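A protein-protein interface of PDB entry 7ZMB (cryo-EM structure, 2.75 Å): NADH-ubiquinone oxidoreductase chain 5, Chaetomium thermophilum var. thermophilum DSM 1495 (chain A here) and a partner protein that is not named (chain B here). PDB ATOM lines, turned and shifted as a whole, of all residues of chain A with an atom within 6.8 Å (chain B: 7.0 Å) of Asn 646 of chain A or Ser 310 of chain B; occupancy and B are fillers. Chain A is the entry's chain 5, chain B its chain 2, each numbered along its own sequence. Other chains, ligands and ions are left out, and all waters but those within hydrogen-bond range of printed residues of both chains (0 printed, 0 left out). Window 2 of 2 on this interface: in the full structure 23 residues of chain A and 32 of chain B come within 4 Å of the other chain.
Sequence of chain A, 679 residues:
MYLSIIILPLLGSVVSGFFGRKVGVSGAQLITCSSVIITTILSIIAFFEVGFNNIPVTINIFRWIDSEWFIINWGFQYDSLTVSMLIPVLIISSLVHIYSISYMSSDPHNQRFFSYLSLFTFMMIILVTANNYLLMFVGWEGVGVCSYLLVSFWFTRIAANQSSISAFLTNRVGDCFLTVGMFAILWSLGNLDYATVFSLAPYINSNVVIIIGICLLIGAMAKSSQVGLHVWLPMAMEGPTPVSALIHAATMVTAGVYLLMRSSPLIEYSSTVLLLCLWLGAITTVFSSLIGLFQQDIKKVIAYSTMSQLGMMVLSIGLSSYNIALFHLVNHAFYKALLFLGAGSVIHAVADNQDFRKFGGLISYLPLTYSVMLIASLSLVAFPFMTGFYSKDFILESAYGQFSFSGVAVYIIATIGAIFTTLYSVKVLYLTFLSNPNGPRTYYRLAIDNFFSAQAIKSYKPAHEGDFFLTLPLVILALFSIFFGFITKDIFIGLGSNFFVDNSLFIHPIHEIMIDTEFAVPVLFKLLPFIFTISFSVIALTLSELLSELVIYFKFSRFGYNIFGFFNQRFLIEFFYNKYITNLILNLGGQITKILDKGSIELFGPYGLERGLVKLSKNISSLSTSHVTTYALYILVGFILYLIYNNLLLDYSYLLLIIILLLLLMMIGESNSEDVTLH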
ATOM      1  N   LEU A 641     -19.521  -9.859 -18.175  1.00  0.00           N
ATOM      2  CA  LEU A 641     -19.223  -8.715 -19.023  1.00  0.00           C
ATOM      3  C   LEU A 641     -18.110  -7.848 -18.451  1.00  0.00           C
ATOM      4  O   LEU A 641     -17.352  -7.243 -19.213  1.00  0.00           O
ATOM      5  CB  LEU A 641     -20.491  -7.889 -19.244  1.00  0.00           C
ATOM      6  CG  LEU A 641     -21.388  -8.379 -20.384  1.00  0.00           C
ATOM      7  CD1 LEU A 641     -22.845  -8.062 -20.128  1.00  0.00           C
ATOM      8  CD2 LEU A 641     -20.929  -7.783 -21.689  1.00  0.00           C
ATOM      9  N   TYR A 642     -17.996  -7.764 -17.122  1.00  0.00           N
ATOM     10  CA  TYR A 642     -16.898  -7.010 -16.527  1.00  0.00           C
ATOM     11  C   TYR A 642     -15.570  -7.715 -16.745  1.00  0.00           C
ATOM     12  O   TYR A 642     -14.540  -7.059 -16.927  1.00  0.00           O
ATOM     13  CB  TYR A 642     -17.134  -6.790 -15.034  1.00  0.00           C
ATOM     14  CG  TYR A 642     -18.016  -5.616 -14.697  1.00  0.00           C
ATOM     15  CD1 TYR A 642     -19.000  -5.185 -15.565  1.00  0.00           C
ATOM     16  CD2 TYR A 642     -17.866  -4.944 -13.500  1.00  0.00           C
ATOM     17  CE1 TYR A 642     -19.810  -4.113 -15.245  1.00  0.00           C
ATOM     18  CE2 TYR A 642     -18.671  -3.884 -13.172  1.00  0.00           C
ATOM     19  CZ  TYR A 642     -19.636  -3.472 -14.050  1.00  0.00           C
ATOM     20  OH  TYR A 642     -20.431  -2.407 -13.728  1.00  0.00           O
ATOM     21  N   LEU A 643     -15.564  -9.049 -16.682  1.00  0.00           N
ATOM     22  CA  LEU A 643     -14.377  -9.799 -17.073  1.00  0.00           C
ATOM     23  C   LEU A 643     -14.056  -9.586 -18.544  1.00  0.00           C
ATOM     24  O   LEU A 643     -12.902  -9.327 -18.898  1.00  0.00           O
ATOM     25  CB  LEU A 643     -14.554 -11.291 -16.773  1.00  0.00           C
ATOM     26  CG  LEU A 643     -14.216 -11.928 -15.415  1.00  0.00           C
ATOM     27  CD1 LEU A 643     -12.737 -11.770 -15.110  1.00  0.00           C
ATOM     28  CD2 LEU A 643     -15.028 -11.367 -14.279  1.00  0.00           C
ATOM     29  N   ILE A 644     -15.065  -9.665 -19.414  1.00  0.00           N
ATOM     30  CA  ILE A 644     -14.843  -9.438 -20.841  1.00  0.00           C
ATOM     31  C   ILE A 644     -14.234  -8.067 -21.070  1.00  0.00           C
ATOM     32  O   ILE A 644     -13.260  -7.919 -21.817  1.00  0.00           O
ATOM     33  CB  ILE A 644     -16.153  -9.591 -21.637  1.00  0.00           C
ATOM     34  CG1 ILE A 644     -16.759 -10.977 -21.476  1.00  0.00           C
ATOM     35  CG2 ILE A 644     -15.906  -9.319 -23.104  1.00  0.00           C
ATOM     36  CD1 ILE A 644     -15.882 -12.054 -21.971  1.00  0.00           C
ATOM     37  N   TYR A 645     -14.796  -7.040 -20.430  1.00  0.00           N
ATOM     38  CA  TYR A 645     -14.308  -5.690 -20.670  1.00  0.00           C
ATOM     39  C   TYR A 645     -12.861  -5.544 -20.235  1.00  0.00           C
ATOM     40  O   TYR A 645     -12.070  -4.868 -20.900  1.00  0.00           O
ATOM     41  CB  TYR A 645     -15.176  -4.663 -19.954  1.00  0.00           C
ATOM     42  CG  TYR A 645     -14.684  -3.253 -20.158  1.00  0.00           C
ATOM     43  CD1 TYR A 645     -14.713  -2.666 -21.414  1.00  0.00           C
ATOM     44  CD2 TYR A 645     -14.169  -2.517 -19.107  1.00  0.00           C
ATOM     45  CE1 TYR A 645     -14.261  -1.378 -21.610  1.00  0.00           C
ATOM     46  CE2 TYR A 645     -13.721  -1.232 -19.291  1.00  0.00           C
ATOM     47  CZ  TYR A 645     -13.767  -0.665 -20.543  1.00  0.00           C
ATOM     48  OH  TYR A 645     -13.315   0.618 -20.727  1.00  0.00           O
ATOM     49  N   ASN A 646     -12.496  -6.176 -19.122  1.00  0.00           N
ATOM     50  CA  ASN A 646     -11.192  -5.921 -18.525  1.00  0.00           C
ATOM     51  C   ASN A 646     -10.067  -6.633 -19.272  1.00  0.00           C
ATOM     52  O   ASN A 646      -9.225  -5.986 -19.899  1.00  0.00           O
ATOM     53  CB  ASN A 646     -11.206  -6.332 -17.052  1.00  0.00           C
ATOM     54  CG  ASN A 646     -10.060  -5.725 -16.274  1.00  0.00           C
ATOM     55  OD1 ASN A 646      -9.641  -4.598 -16.540  1.00  0.00           O
ATOM     56  ND2 ASN A 646      -9.545  -6.468 -15.303  1.00  0.00           N
ATOM     57  N   ASN A 647     -10.047  -7.965 -19.236  1.00  0.00           N
ATOM     58  CA  ASN A 647      -8.836  -8.669 -19.648  1.00  0.00           C
ATOM     59  C   ASN A 647      -8.734  -8.772 -21.164  1.00  0.00           C
ATOM     60  O   ASN A 647      -7.653  -9.049 -21.697  1.00  0.00           O
ATOM     61  CB  ASN A 647      -8.772 -10.051 -19.002  1.00  0.00           C
ATOM     62  CG  ASN A 647      -9.711 -11.041 -19.641  1.00  0.00           C
ATOM     63  OD1 ASN A 647     -10.901 -10.782 -19.785  1.00  0.00           O
ATOM     64  ND2 ASN A 647      -9.176 -12.192 -20.030  1.00  0.00           N
ATOM     65  N   LEU A 648      -9.835  -8.550 -21.879  1.00  0.00           N
ATOM     66  CA  LEU A 648      -9.731  -8.452 -23.330  1.00  0.00           C
ATOM     67  C   LEU A 648      -9.080  -7.155 -23.776  1.00  0.00           C
ATOM     68  O   LEU A 648      -8.674  -7.056 -24.937  1.00  0.00           O
ATOM     69  CB  LEU A 648     -11.104  -8.572 -23.988  1.00  0.00           C
ATOM     70  CG  LEU A 648     -11.674  -9.971 -24.228  1.00  0.00           C
ATOM     71  CD1 LEU A 648     -10.802 -10.743 -25.211  1.00  0.00           C
ATOM     72  CD2 LEU A 648     -11.847 -10.736 -22.929  1.00  0.00           C
ATOM     73  N   LEU A 649      -8.960  -6.176 -22.876  1.00  0.00           N
ATOM     74  CA  LEU A 649      -8.460  -4.845 -23.204  1.00  0.00           C
ATOM     75  C   LEU A 649      -9.287  -4.231 -24.331  1.00  0.00           C
ATOM     76  O   LEU A 649      -8.764  -3.671 -25.296  1.00  0.00           O
ATOM     77  CB  LEU A 649      -6.969  -4.884 -23.555  1.00  0.00           C
ATOM     78  CG  LEU A 649      -6.236  -3.540 -23.565  1.00  0.00           C
ATOM     79  CD1 LEU A 649      -6.475  -2.802 -22.260  1.00  0.00           C
ATOM     80  CD2 LEU A 649      -4.749  -3.739 -23.810  1.00  0.00           C
ATOM     81  N   LEU A 650     -10.602  -4.367 -24.207  1.00  0.00           N
ATOM     82  CA  LEU A 650     -11.502  -3.770 -25.178  1.00  0.00           C
ATOM     83  C   LEU A 650     -11.349  -2.256 -25.177  1.00  0.00           C
ATOM     84  O   LEU A 650     -11.101  -1.634 -24.140  1.00  0.00           O
ATOM     85  CB  LEU A 650     -12.951  -4.140 -24.865  1.00  0.00           C
ATOM     86  CG  LEU A 650     -13.364  -5.603 -24.947  1.00  0.00           C
ATOM     87  CD1 LEU A 650     -14.872  -5.721 -24.830  1.00  0.00           C
ATOM     88  CD2 LEU A 650     -12.873  -6.230 -26.240  1.00  0.00           C
ATOM     89  N   TYR B 238      -0.237  -9.526 -13.233  1.00  0.00           N
ATOM     90  CA  TYR B 238      -1.610  -9.393 -13.781  1.00  0.00           C
ATOM     91  C   TYR B 238      -2.665  -9.754 -12.733  1.00  0.00           C
ATOM     92  O   TYR B 238      -3.718  -9.119 -12.715  1.00  0.00           O
ATOM     93  CB  TYR B 238      -1.741 -10.142 -15.106  1.00  0.00           C
ATOM     94  CG  TYR B 238      -1.101  -9.441 -16.275  1.00  0.00           C
ATOM     95  CD1 TYR B 238      -1.609  -8.246 -16.751  1.00  0.00           C
ATOM     96  CD2 TYR B 238       0.011  -9.973 -16.903  1.00  0.00           C
ATOM     97  CE1 TYR B 238      -1.027  -7.595 -17.826  1.00  0.00           C
ATOM     98  CE2 TYR B 238       0.603  -9.337 -17.981  1.00  0.00           C
ATOM     99  CZ  TYR B 238       0.083  -8.142 -18.443  1.00  0.00           C
ATOM    100  OH  TYR B 238       0.666  -7.510 -19.502  1.00  0.00           O
ATOM    101  N   ASN B 241      -4.807  -6.813 -10.441  1.00  0.00           N
ATOM    102  CA  ASN B 241      -5.932  -6.023 -10.999  1.00  0.00           C
ATOM    103  C   ASN B 241      -7.142  -6.918 -11.248  1.00  0.00           C
ATOM    104  O   ASN B 241      -8.249  -6.487 -10.942  1.00  0.00           O
ATOM    105  CB  ASN B 241      -5.512  -5.173 -12.200  1.00  0.00           C
ATOM    106  CG  ASN B 241      -4.966  -3.817 -11.816  1.00  0.00           C
ATOM    107  OD1 ASN B 241      -5.480  -3.170 -10.908  1.00  0.00           O
ATOM    108  ND2 ASN B 241      -3.937  -3.375 -12.515  1.00  0.00           N
ATOM    109  N   PHE B 242      -6.961  -8.128 -11.780  1.00  0.00           N
ATOM    110  CA  PHE B 242      -8.182  -8.893 -11.966  1.00  0.00           C
ATOM    111  C   PHE B 242      -8.518  -9.885 -10.858  1.00  0.00           C
ATOM    112  O   PHE B 242      -9.582 -10.498 -10.928  1.00  0.00           O
ATOM    113  CB  PHE B 242      -8.233  -9.576 -13.344  1.00  0.00           C
ATOM    114  CG  PHE B 242      -7.065 -10.449 -13.681  1.00  0.00           C
ATOM    115  CD1 PHE B 242      -6.906 -11.675 -13.118  1.00  0.00           C
ATOM    116  CD2 PHE B 242      -6.048  -9.963 -14.476  1.00  0.00           C
ATOM    117  CE1 PHE B 242      -5.805 -12.474 -13.428  1.00  0.00           C
ATOM    118  CE2 PHE B 242      -4.976 -10.758 -14.823  1.00  0.00           C
ATOM    119  CZ  PHE B 242      -4.840 -12.006 -14.276  1.00  0.00           C
ATOM    120  N   SER B 243      -7.695 -10.044  -9.826  1.00  0.00           N
ATOM    121  CA  SER B 243      -8.254 -10.607  -8.599  1.00  0.00           C
ATOM    122  C   SER B 243      -9.093  -9.567  -7.876  1.00  0.00           C
ATOM    123  O   SER B 243     -10.161  -9.882  -7.341  1.00  0.00           O
ATOM    124  CB  SER B 243      -7.158 -11.125  -7.670  1.00  0.00           C
ATOM    125  OG  SER B 243      -6.485 -12.228  -8.234  1.00  0.00           O
ATOM    126  N   LEU B 245     -10.737  -7.266  -9.270  1.00  0.00           N
ATOM    127  CA  LEU B 245     -11.963  -7.068 -10.034  1.00  0.00           C
ATOM    128  C   LEU B 245     -13.078  -7.974  -9.534  1.00  0.00           C
ATOM    129  O   LEU B 245     -14.208  -7.524  -9.317  1.00  0.00           O
ATOM    130  CB  LEU B 245     -11.695  -7.325 -11.514  1.00  0.00           C
ATOM    131  CG  LEU B 245     -12.850  -7.110 -12.495  1.00  0.00           C
ATOM    132  CD1 LEU B 245     -13.285  -5.669 -12.528  1.00  0.00           C
ATOM    133  CD2 LEU B 245     -12.500  -7.605 -13.876  1.00  0.00           C
ATOM    134  N   THR B 298      -3.568   1.011  -4.437  1.00  0.00           N
ATOM    135  CA  THR B 298      -3.372   0.200  -5.665  1.00  0.00           C
ATOM    136  C   THR B 298      -3.284   1.068  -6.927  1.00  0.00           C
ATOM    137  O   THR B 298      -3.381   0.492  -8.018  1.00  0.00           O
ATOM    138  CB  THR B 298      -4.420  -0.910  -5.798  1.00  0.00           C
ATOM    139  OG1 THR B 298      -5.722  -0.324  -5.811  1.00  0.00           O
ATOM    140  CG2 THR B 298      -4.307  -1.960  -4.715  1.00  0.00           C
ATOM    141  N   ASN B 299      -3.135   2.389  -6.795  1.00  0.00           N
ATOM    142  CA  ASN B 299      -3.124   3.254  -8.005  1.00  0.00           C
ATOM    143  C   ASN B 299      -1.694   3.390  -8.507  1.00  0.00           C
ATOM    144  O   ASN B 299      -0.852   3.902  -7.742  1.00  0.00           O
ATOM    145  CB  ASN B 299      -3.671   4.653  -7.750  1.00  0.00           C
ATOM    146  CG  ASN B 299      -4.942   4.949  -8.515  1.00  0.00           C
ATOM    147  OD1 ASN B 299      -5.420   4.113  -9.273  1.00  0.00           O
ATOM    148  ND2 ASN B 299      -5.491   6.137  -8.329  1.00  0.00           N
ATOM    149  N   SER B 300      -1.452   2.993  -9.757  1.00  0.00           N
ATOM    150  CA  SER B 300      -0.098   3.104 -10.355  1.00  0.00           C
ATOM    151  C   SER B 300       0.151   4.541 -10.813  1.00  0.00           C
ATOM    152  O   SER B 300      -0.420   4.924 -11.848  1.00  0.00           O
ATOM    153  CB  SER B 300       0.056   2.148 -11.505  1.00  0.00           C
ATOM    154  OG  SER B 300      -0.082   0.805 -11.069  1.00  0.00           O
ATOM    155  N   TYR B 305       1.422  -1.008 -18.183  1.00  0.00           N
ATOM    156  CA  TYR B 305       0.539  -2.078 -18.714  1.00  0.00           C
ATOM    157  C   TYR B 305      -0.478  -2.442 -17.627  1.00  0.00           C
ATOM    158  O   TYR B 305      -1.642  -2.717 -17.966  1.00  0.00           O
ATOM    159  CB  TYR B 305       1.367  -3.272 -19.201  1.00  0.00           C
ATOM    160  CG  TYR B 305       2.262  -3.917 -18.170  1.00  0.00           C
ATOM    161  CD1 TYR B 305       1.910  -5.115 -17.571  1.00  0.00           C
ATOM    162  CD2 TYR B 305       3.470  -3.345 -17.807  1.00  0.00           C
ATOM    163  CE1 TYR B 305       2.727  -5.722 -16.632  1.00  0.00           C
ATOM    164  CE2 TYR B 305       4.296  -3.936 -16.865  1.00  0.00           C
ATOM    165  CZ  TYR B 305       3.924  -5.130 -16.276  1.00  0.00           C
ATOM    166  OH  TYR B 305       4.736  -5.718 -15.351  1.00  0.00           O
ATOM    167  N   LEU B 306      -0.051  -2.432 -16.362  1.00  0.00           N
ATOM    168  CA  LEU B 306      -0.975  -2.720 -15.235  1.00  0.00           C
ATOM    169  C   LEU B 306      -2.092  -1.671 -15.215  1.00  0.00           C
ATOM    170  O   LEU B 306      -3.245  -2.050 -14.948  1.00  0.00           O
ATOM    171  CB  LEU B 306      -0.179  -2.684 -13.929  1.00  0.00           C
ATOM    172  CG  LEU B 306       0.973  -3.681 -13.848  1.00  0.00           C
ATOM    173  CD1 LEU B 306       1.798  -3.451 -12.593  1.00  0.00           C
ATOM    174  CD2 LEU B 306       0.447  -5.107 -13.898  1.00  0.00           C
ATOM    175  N   SER B 307      -1.763  -0.408 -15.493  1.00  0.00           N
ATOM    176  CA  SER B 307      -2.776   0.678 -15.436  1.00  0.00           C
ATOM    177  C   SER B 307      -3.889   0.391 -16.447  1.00  0.00           C
ATOM    178  O   SER B 307      -5.058   0.687 -16.136  1.00  0.00           O
ATOM    179  CB  SER B 307      -2.145   2.025 -15.678  1.00  0.00           C
ATOM    180  OG  SER B 307      -3.126   3.051 -15.666  1.00  0.00           O
ATOM    181  N   GLU B 308      -3.532  -0.143 -17.616  1.00  0.00           N
ATOM    182  CA  GLU B 308      -4.534  -0.428 -18.674  1.00  0.00           C
ATOM    183  C   GLU B 308      -5.591  -1.403 -18.152  1.00  0.00           C
ATOM    184  O   GLU B 308      -6.695  -1.426 -18.721  1.00  0.00           O
ATOM    185  CB  GLU B 308      -3.840  -1.030 -19.895  1.00  0.00           C
ATOM    186  CG  GLU B 308      -2.773  -0.129 -20.484  1.00  0.00           C
ATOM    187  CD  GLU B 308      -3.297   1.170 -21.072  1.00  0.00           C
ATOM    188  OE1 GLU B 308      -2.576   2.185 -20.990  1.00  0.00           O
ATOM    189  OE2 GLU B 308      -4.418   1.163 -21.619  1.00  0.00           O
ATOM    190  N   PHE B 309      -5.269  -2.177 -17.115  1.00  0.00           N
ATOM    191  CA  PHE B 309      -6.222  -3.189 -16.680  1.00  0.00           C
ATOM    192  C   PHE B 309      -6.732  -2.943 -15.265  1.00  0.00           C
ATOM    193  O   PHE B 309      -7.040  -3.898 -14.548  1.00  0.00           O
ATOM    194  CB  PHE B 309      -5.593  -4.579 -16.759  1.00  0.00           C
ATOM    195  CG  PHE B 309      -5.247  -5.013 -18.143  1.00  0.00           C
ATOM    196  CD1 PHE B 309      -6.229  -5.461 -19.011  1.00  0.00           C
ATOM    197  CD2 PHE B 309      -3.935  -4.986 -18.582  1.00  0.00           C
ATOM    198  CE1 PHE B 309      -5.910  -5.864 -20.290  1.00  0.00           C
ATOM    199  CE2 PHE B 309      -3.608  -5.390 -19.859  1.00  0.00           C
ATOM    200  CZ  PHE B 309      -4.596  -5.830 -20.714  1.00  0.00           C
ATOM    201  N   SER B 310      -6.832  -1.686 -14.849  1.00  0.00           N
ATOM    202  CA  SER B 310      -7.121  -1.390 -13.455  1.00  0.00           C
ATOM    203  C   SER B 310      -8.478  -1.947 -13.046  1.00  0.00           C
ATOM    204  O   SER B 310      -9.473  -1.798 -13.755  1.00  0.00           O
ATOM    205  CB  SER B 310      -7.070   0.113 -13.208  1.00  0.00           C
ATOM    206  OG  SER B 310      -7.396   0.414 -11.868  1.00  0.00           O
ATOM    207  N   TRP B 311      -8.507  -2.595 -11.886  1.00  0.00           N
ATOM    208  CA  TRP B 311      -9.758  -3.094 -11.346  1.00  0.00           C
ATOM    209  C   TRP B 311     -10.742  -1.968 -11.076  1.00  0.00           C
ATOM    210  O   TRP B 311     -11.943  -2.222 -10.957  1.00  0.00           O
ATOM    211  CB  TRP B 311      -9.486  -3.870 -10.066  1.00  0.00           C
ATOM    212  CG  TRP B 311      -9.144  -2.986  -8.931  1.00  0.00           C
ATOM    213  CD1 TRP B 311      -7.934  -2.440  -8.655  1.00  0.00           C
ATOM    214  CD2 TRP B 311     -10.036  -2.520  -7.924  1.00  0.00           C
ATOM    215  NE1 TRP B 311      -8.011  -1.670  -7.529  1.00  0.00           N
ATOM    216  CE2 TRP B 311      -9.296  -1.703  -7.060  1.00  0.00           C
ATOM    217  CE3 TRP B 311     -11.392  -2.718  -7.668  1.00  0.00           C
ATOM    218  CZ2 TRP B 311      -9.867  -1.078  -5.965  1.00  0.00           C
ATOM    219  CZ3 TRP B 311     -11.951  -2.102  -6.576  1.00  0.00           C
ATOM    220  CH2 TRP B 311     -11.189  -1.298  -5.732  1.00  0.00           C
ATOM    221  N   THR B 312     -10.259  -0.733 -10.977  1.00  0.00           N
ATOM    222  CA  THR B 312     -11.131   0.394 -10.701  1.00  0.00           C
ATOM    223  C   THR B 312     -11.982   0.803 -11.893  1.00  0.00           C
ATOM    224  O   THR B 312     -12.849   1.663 -11.734  1.00  0.00           O
ATOM    225  CB  THR B 312     -10.312   1.588 -10.211  1.00  0.00           C
ATOM    226  OG1 THR B 312      -9.395   2.004 -11.227  1.00  0.00           O
ATOM    227  CG2 THR B 312      -9.554   1.221  -8.973  1.00  0.00           C
ATOM    228  N   TYR B 313     -11.773   0.218 -13.075  1.00  0.00           N
ATOM    229  CA  TYR B 313     -12.653   0.562 -14.185  1.00  0.00           C
ATOM    230  C   TYR B 313     -14.033  -0.049 -14.014  1.00  0.00           C
ATOM    231  O   TYR B 313     -15.006   0.478 -14.554  1.00  0.00           O
ATOM    232  CB  TYR B 313     -12.049   0.160 -15.525  1.00  0.00           C
ATOM    233  CG  TYR B 313     -10.737   0.847 -15.777  1.00  0.00           C
ATOM    234  CD1 TYR B 313     -10.672   2.226 -15.884  1.00  0.00           C
ATOM    235  CD2 TYR B 313      -9.583   0.121 -15.993  1.00  0.00           C
ATOM    236  CE1 TYR B 313      -9.475   2.865 -16.119  1.00  0.00           C
ATOM    237  CE2 TYR B 313      -8.387   0.750 -16.239  1.00  0.00           C
ATOM    238  CZ  TYR B 313      -8.335   2.122 -16.300  1.00  0.00           C
ATOM    239  OH  TYR B 313      -7.137   2.742 -16.551  1.00  0.00           O
ATOM    240  N   ALA B 314     -14.146  -1.130 -13.246  1.00  0.00           N
ATOM    241  CA  ALA B 314     -15.464  -1.601 -12.847  1.00  0.00           C
ATOM    242  C   ALA B 314     -16.229  -0.515 -12.113  1.00  0.00           C
ATOM    243  O   ALA B 314     -17.433  -0.344 -12.323  1.00  0.00           O
ATOM    244  CB  ALA B 314     -15.342  -2.839 -11.970  1.00  0.00           C
ATOM    245  N   LEU B 315     -15.545   0.230 -11.246  1.00  0.00           N
ATOM    246  CA  LEU B 315     -16.205   1.285 -10.493  1.00  0.00           C
ATOM    247  C   LEU B 315     -16.727   2.382 -11.411  1.00  0.00           C
ATOM    248  O   LEU B 315     -17.843   2.873 -11.215  1.00  0.00           O
ATOM    249  CB  LEU B 315     -15.255   1.860  -9.449  1.00  0.00           C
ATOM    250  CG  LEU B 315     -14.766   0.957  -8.319  1.00  0.00           C
ATOM    251  CD1 LEU B 315     -14.267   1.805  -7.161  1.00  0.00           C
ATOM    252  CD2 LEU B 315     -15.844  -0.017  -7.866  1.00  0.00           C
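Hydrophobic or aromatic side chains of chain A that line the printed part of chain B: Tyr 642 and Leu 649. Of the 19 printed residues of chain B, 6 touch a printed residue of chain A. Among the printed residues, no Asp or Glu carboxylate lies within 4 Å of a Lys or Arg side-chain nitrogen of the other chain.
The side-chain amide oxygen of Asn 646 of chain A sits close to the backbone carbonyl oxygen of Phe 309 of chain B, at 3.4 Å.
Asn 646 of chain A touches just these residues of chain B: Phe 242 (3.9 Å), Leu 245 (3.5 Å), Phe 309 (3.2 Å) and Ser 310 (3.95 Å). Printed residues of chain A within 4 Å of Phe 242 of chain B: Asn 646. Ser 300 of chain B touches none of the printed residues of chain A. Of chain A, only Asn 646 comes within 4 Å of Ser 310 of chain B. Of the printed residues of chain A, Ala 314 of chain B touches Tyr 642 (3.6 Å). The nearest printed residue of chain A that does not touch Ser 310 of chain B is Tyr 645 of chain A (7.0 Å). The nearest printed residue of chain A that does not touch Leu 245 of chain B is Leu 643 of chain A (4.3 Å).
The side-chain hydroxyl (OG) of Ser 310 of chain B sits at hydrogen-bond distance from the side-chain hydroxyl (OG1) of Thr 312 of chain B (2.6 Å). The backbone carbonyl oxygen (O) of Leu 643 of chain A lies close to the side-chain amide oxygen (OD1) of Asn 647 of chain A, 2.6 Å away.
Among the printed residues, merely in contact across the chains: Tyr 642 of chain A with Leu 245 of chain B, Tyr 642 of chain A with Ala 314 of chain B, Asn 646 of chain A with Phe 242 of chain B, Asn 646 of chain A with Leu 245 of chain B, Asn 646 of chain A with Ser 310 of chain B, Asn 647 of chain A with Phe 309 of chain B, Leu 649 of chain A with Glu 308 of chain B and Leu 649 of chain A with Phe 309 of chain B.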
